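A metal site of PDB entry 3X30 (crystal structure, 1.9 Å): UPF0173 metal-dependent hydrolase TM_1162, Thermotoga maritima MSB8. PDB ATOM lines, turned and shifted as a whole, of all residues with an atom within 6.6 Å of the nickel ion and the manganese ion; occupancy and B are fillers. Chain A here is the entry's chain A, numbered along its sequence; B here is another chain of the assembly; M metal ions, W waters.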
ATOM      1  N   HIS A   9      22.530 -34.814  -9.150  1.00  0.00           N
ATOM      2  CA  HIS A   9      21.562 -33.881  -8.553  1.00  0.00           C
ATOM      3  C   HIS A   9      21.293 -34.234  -7.080  1.00  0.00           C
ATOM      4  O   HIS A   9      22.151 -34.006  -6.236  1.00  0.00           O
ATOM      5  CB  HIS A   9      20.267 -33.813  -9.374  1.00  0.00           C
ATOM      6  CG  HIS A   9      19.501 -32.541  -9.164  1.00  0.00           C
ATOM      7  ND1 HIS A   9      20.064 -31.291  -9.331  1.00  0.00           N
ATOM      8  CD2 HIS A   9      18.213 -32.324  -8.786  1.00  0.00           C
ATOM      9  CE1 HIS A   9      19.165 -30.370  -9.067  1.00  0.00           C
ATOM     10  NE2 HIS A   9      18.029 -30.959  -8.739  1.00  0.00           N
ATOM     11  N   ALA A  10      20.118 -34.792  -6.760  1.00  0.00           N
ATOM     12  CA  ALA A  10      19.839 -35.199  -5.369  1.00  0.00           C
ATOM     13  C   ALA A  10      19.514 -36.694  -5.261  1.00  0.00           C
ATOM     14  O   ALA A  10      19.009 -37.162  -4.231  1.00  0.00           O
ATOM     15  CB  ALA A  10      18.691 -34.369  -4.776  1.00  0.00           C
ATOM     16  N   HIS A  49      10.438 -33.568  -1.264  1.00  0.00           N
ATOM     17  CA  HIS A  49       9.452 -32.526  -1.525  1.00  0.00           C
ATOM     18  C   HIS A  49       8.916 -32.640  -2.943  1.00  0.00           C
ATOM     19  O   HIS A  49       9.397 -33.456  -3.726  1.00  0.00           O
ATOM     20  CB  HIS A  49      10.038 -31.122  -1.242  1.00  0.00           C
ATOM     21  CG  HIS A  49      11.145 -30.694  -2.168  1.00  0.00           C
ATOM     22  ND1 HIS A  49      12.346 -31.374  -2.269  1.00  0.00           N
ATOM     23  CD2 HIS A  49      11.263 -29.616  -2.973  1.00  0.00           C
ATOM     24  CE1 HIS A  49      13.146 -30.734  -3.106  1.00  0.00           C
ATOM     25  NE2 HIS A  49      12.501 -29.671  -3.565  1.00  0.00           N
ATOM     26  N   HIS A  51       8.883 -30.777  -5.728  1.00  0.00           N
ATOM     27  CA  HIS A  51       9.528 -30.234  -6.935  1.00  0.00           C
ATOM     28  C   HIS A  51       9.967 -31.360  -7.872  1.00  0.00           C
ATOM     29  O   HIS A  51      10.451 -32.416  -7.425  1.00  0.00           O
ATOM     30  CB  HIS A  51      10.732 -29.353  -6.551  1.00  0.00           C
ATOM     31  CG  HIS A  51      10.346 -28.112  -5.808  1.00  0.00           C
ATOM     32  ND1 HIS A  51      11.248 -27.327  -5.129  1.00  0.00           N
ATOM     33  CD2 HIS A  51       9.131 -27.529  -5.624  1.00  0.00           C
ATOM     34  CE1 HIS A  51      10.619 -26.323  -4.551  1.00  0.00           C
ATOM     35  NE2 HIS A  51       9.329 -26.425  -4.831  1.00  0.00           N
ATOM     36  N   ASP A  53      12.335 -32.111  -9.863  1.00  0.00           N
ATOM     37  CA  ASP A  53      13.715 -32.615  -9.897  1.00  0.00           C
ATOM     38  C   ASP A  53      14.021 -33.469  -8.667  1.00  0.00           C
ATOM     39  O   ASP A  53      15.172 -33.858  -8.435  1.00  0.00           O
ATOM     40  CB  ASP A  53      14.717 -31.458 -10.018  1.00  0.00           C
ATOM     41  CG  ASP A  53      14.552 -30.386  -8.947  1.00  0.00           C
ATOM     42  OD1 ASP A  53      13.401 -29.976  -8.645  1.00  0.00           O
ATOM     43  OD2 ASP A  53      15.586 -29.952  -8.390  1.00  0.00           O
ATOM     44  N   HIS A  54      12.979 -33.785  -7.891  1.00  0.00           N
ATOM     45  CA  HIS A  54      13.111 -34.665  -6.727  1.00  0.00           C
ATOM     46  C   HIS A  54      12.057 -35.750  -6.776  1.00  0.00           C
ATOM     47  O   HIS A  54      12.384 -36.925  -6.693  1.00  0.00           O
ATOM     48  CB  HIS A  54      13.019 -33.874  -5.434  1.00  0.00           C
ATOM     49  CG  HIS A  54      14.119 -32.872  -5.290  1.00  0.00           C
ATOM     50  ND1 HIS A  54      15.241 -33.101  -4.530  1.00  0.00           N
ATOM     51  CD2 HIS A  54      14.302 -31.671  -5.894  1.00  0.00           C
ATOM     52  CE1 HIS A  54      16.066 -32.066  -4.642  1.00  0.00           C
ATOM     53  NE2 HIS A  54      15.516 -31.192  -5.465  1.00  0.00           N
ATOM     54  N   HIS A 109      12.252 -24.478   2.671  1.00  0.00           N
ATOM     55  CA  HIS A 109      12.182 -24.609   1.219  1.00  0.00           C
ATOM     56  C   HIS A 109      10.703 -24.499   0.828  1.00  0.00           C
ATOM     57  O   HIS A 109       9.913 -23.905   1.580  1.00  0.00           O
ATOM     58  CB  HIS A 109      12.815 -25.962   0.771  1.00  0.00           C
ATOM     59  CG  HIS A 109      13.099 -26.070  -0.694  1.00  0.00           C
ATOM     60  ND1 HIS A 109      14.025 -25.281  -1.338  1.00  0.00           N
ATOM     61  CD2 HIS A 109      12.594 -26.897  -1.647  1.00  0.00           C
ATOM     62  CE1 HIS A 109      14.070 -25.607  -2.621  1.00  0.00           C
ATOM     63  NE2 HIS A 109      13.208 -26.584  -2.834  1.00  0.00           N
ATOM     64  N   GLY A 110      10.326 -25.062  -0.317  1.00  0.00           N
ATOM     65  CA  GLY A 110       8.923 -25.144  -0.700  1.00  0.00           C
ATOM     66  C   GLY A 110       8.601 -26.547  -1.159  1.00  0.00           C
ATOM     67  O   GLY A 110       9.502 -27.382  -1.267  1.00  0.00           O
ATOM     68  N   ASP A 142      16.112 -30.475  -0.507  1.00  0.00           N
ATOM     69  CA  ASP A 142      16.385 -29.065  -0.791  1.00  0.00           C
ATOM     70  C   ASP A 142      16.122 -28.262   0.471  1.00  0.00           C
ATOM     71  O   ASP A 142      15.065 -28.375   1.079  1.00  0.00           O
ATOM     72  CB  ASP A 142      15.513 -28.511  -1.900  1.00  0.00           C
ATOM     73  CG  ASP A 142      16.003 -28.845  -3.297  1.00  0.00           C
ATOM     74  OD1 ASP A 142      17.083 -29.454  -3.457  1.00  0.00           O
ATOM     75  OD2 ASP A 142      15.263 -28.485  -4.240  1.00  0.00           O
ATOM     76  N   PHE A 168      18.449 -21.887  -5.205  1.00  0.00           N
ATOM     77  CA  PHE A 168      17.289 -22.609  -4.665  1.00  0.00           C
ATOM     78  C   PHE A 168      17.608 -23.250  -3.323  1.00  0.00           C
ATOM     79  O   PHE A 168      16.689 -23.599  -2.565  1.00  0.00           O
ATOM     80  CB  PHE A 168      16.808 -23.704  -5.603  1.00  0.00           C
ATOM     81  CG  PHE A 168      16.291 -23.186  -6.918  1.00  0.00           C
ATOM     82  CD1 PHE A 168      15.123 -22.455  -6.983  1.00  0.00           C
ATOM     83  CD2 PHE A 168      16.999 -23.418  -8.091  1.00  0.00           C
ATOM     84  CE1 PHE A 168      14.643 -21.972  -8.201  1.00  0.00           C
ATOM     85  CE2 PHE A 168      16.528 -22.948  -9.302  1.00  0.00           C
ATOM     86  CZ  PHE A 168      15.355 -22.224  -9.362  1.00  0.00           C
ATOM     87  N   VAL A 169      18.885 -23.434  -3.046  1.00  0.00           N
ATOM     88  CA  VAL A 169      19.343 -24.149  -1.859  1.00  0.00           C
ATOM     89  C   VAL A 169      20.585 -23.476  -1.315  1.00  0.00           C
ATOM     90  O   VAL A 169      21.069 -22.511  -1.914  1.00  0.00           O
ATOM     91  CB  VAL A 169      19.669 -25.629  -2.170  1.00  0.00           C
ATOM     92  CG1 VAL A 169      18.418 -26.365  -2.696  1.00  0.00           C
ATOM     93  CG2 VAL A 169      20.810 -25.706  -3.172  1.00  0.00           C
ATOM     94  N   HIS A 191      23.321 -31.709  -5.370  1.00  0.00           N
ATOM     95  CA  HIS A 191      22.462 -30.671  -5.925  1.00  0.00           C
ATOM     96  C   HIS A 191      23.301 -29.490  -6.410  1.00  0.00           C
ATOM     97  O   HIS A 191      23.065 -28.341  -6.042  1.00  0.00           O
ATOM     98  CB  HIS A 191      21.429 -30.218  -4.870  1.00  0.00           C
ATOM     99  CG  HIS A 191      20.200 -29.598  -5.453  1.00  0.00           C
ATOM    100  ND1 HIS A 191      20.139 -28.282  -5.875  1.00  0.00           N
ATOM    101  CD2 HIS A 191      18.965 -30.118  -5.673  1.00  0.00           C
ATOM    102  CE1 HIS A 191      18.926 -28.016  -6.325  1.00  0.00           C
ATOM    103  NE2 HIS A 191      18.195 -29.121  -6.211  1.00  0.00           N
ATOM    104  N   TRP A 195      22.510 -27.814 -13.532  1.00  0.00           N
ATOM    105  CA  TRP A 195      22.282 -26.695 -14.452  1.00  0.00           C
ATOM    106  C   TRP A 195      23.218 -25.553 -14.068  1.00  0.00           C
ATOM    107  O   TRP A 195      23.761 -25.540 -12.967  1.00  0.00           O
ATOM    108  CB  TRP A 195      20.818 -26.234 -14.414  1.00  0.00           C
ATOM    109  CG  TRP A 195      19.871 -27.319 -14.767  1.00  0.00           C
ATOM    110  CD1 TRP A 195      19.575 -27.787 -16.018  1.00  0.00           C
ATOM    111  CD2 TRP A 195      19.071 -28.082 -13.856  1.00  0.00           C
ATOM    112  NE1 TRP A 195      18.648 -28.797 -15.936  1.00  0.00           N
ATOM    113  CE2 TRP A 195      18.316 -28.993 -14.621  1.00  0.00           C
ATOM    114  CE3 TRP A 195      18.910 -28.067 -12.471  1.00  0.00           C
ATOM    115  CZ2 TRP A 195      17.423 -29.897 -14.050  1.00  0.00           C
ATOM    116  CZ3 TRP A 195      18.016 -28.971 -11.900  1.00  0.00           C
ATOM    117  CH2 TRP A 195      17.292 -29.859 -12.684  1.00  0.00           C
ATOM    118  N   TYR B  73      10.065 -20.252  -5.931  1.00  0.00           N
ATOM    119  CA  TYR B  73       9.736 -20.963  -7.144  1.00  0.00           C
ATOM    120  C   TYR B  73       8.244 -20.928  -7.441  1.00  0.00           C
ATOM    121  O   TYR B  73       7.833 -20.668  -8.569  1.00  0.00           O
ATOM    122  CB  TYR B  73      10.249 -22.404  -7.023  1.00  0.00           C
ATOM    123  CG  TYR B  73       9.763 -23.384  -8.073  1.00  0.00           C
ATOM    124  CD1 TYR B  73      10.232 -23.331  -9.376  1.00  0.00           C
ATOM    125  CD2 TYR B  73       8.882 -24.404  -7.724  1.00  0.00           C
ATOM    126  CE1 TYR B  73       9.808 -24.272 -10.321  1.00  0.00           C
ATOM    127  CE2 TYR B  73       8.455 -25.322  -8.642  1.00  0.00           C
ATOM    128  CZ  TYR B  73       8.913 -25.256  -9.936  1.00  0.00           C
ATOM    129  OH  TYR B  73       8.451 -26.204 -10.829  1.00  0.00           O
ATOM    130  N   HIS B  90      14.770 -19.990  -3.678  1.00  0.00           N
ATOM    131  CA  HIS B  90      13.958 -20.488  -2.567  1.00  0.00           C
ATOM    132  C   HIS B  90      14.663 -20.249  -1.235  1.00  0.00           C
ATOM    133  O   HIS B  90      15.749 -19.645  -1.191  1.00  0.00           O
ATOM    134  CB  HIS B  90      13.558 -21.969  -2.726  1.00  0.00           C
ATOM    135  CG  HIS B  90      12.106 -22.195  -2.391  1.00  0.00           C
ATOM    136  ND1 HIS B  90      11.194 -22.659  -3.318  1.00  0.00           N
ATOM    137  CD2 HIS B  90      11.398 -21.888  -1.284  1.00  0.00           C
ATOM    138  CE1 HIS B  90       9.997 -22.688  -2.768  1.00  0.00           C
ATOM    139  NE2 HIS B  90      10.089 -22.211  -1.542  1.00  0.00           N
HETATM  140 NI    NI M   1      13.256 -27.856  -4.552  1.00  0.00          NI
HETATM  141 MN    MN M   2      15.923 -29.165  -6.152  1.00  0.00          MN
HETATM  142  O   HOH W   1      13.774 -28.674  -6.542  1.00  0.00           O
HETATM  143  O   HOH W   2      16.148 -26.927  -6.984  1.00  0.00           O
HETATM  144  O   HOH W   3      14.049 -26.118  -5.705  1.00  0.00           O
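O of Phe 168 lies close to ND1 of His 109 (3.4 Å). N of His 191 sits at hydrogen-bond distance from O of His 9, 2.7 Å away. The side-chain carboxylate (OD2) of Asp 53 sits close to a ring nitrogen (NE2) of His 9 (2.7 Å).
The manganese ion is bound by OD2 of Asp 142 (2.1 Å), NE2 of His 54 (2.2 Å), water W1 (2.2 Å), NE2 of His 191 (2.3 Å), OD2 of Asp 53 (2.4 Å) and water W2 (2.4 Å). The manganese ion has six donor atoms within binding distance. Slightly farther from the manganese ion lies the side-chain carboxylate (OD1) of Asp 142 (2.9 Å).
Four residues have an atom within 4 Å of the nickel ion: His 49, His 51, His 109 and Asp 142. Along chain A the residues within 4 Å of the nickel ion span positions 49 to 142.
NE2 of His 9 touches the manganese ion, at 3.8 Å. Within 4 Å of the manganese ion: His 9, Asp 53, His 54, Asp 142 and His 191.
The nickel ion is bound by the side-chain carboxylate (OD2) of Asp 142 (2.1 Å), a ring nitrogen (NE2) of His 109 (2.1 Å), a ring nitrogen (ND1) of His 51 (2.2 Å), a ring nitrogen (NE2) of His 49 (2.2 Å), water W1 (2.2 Å) and water W3 (2.2 Å).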
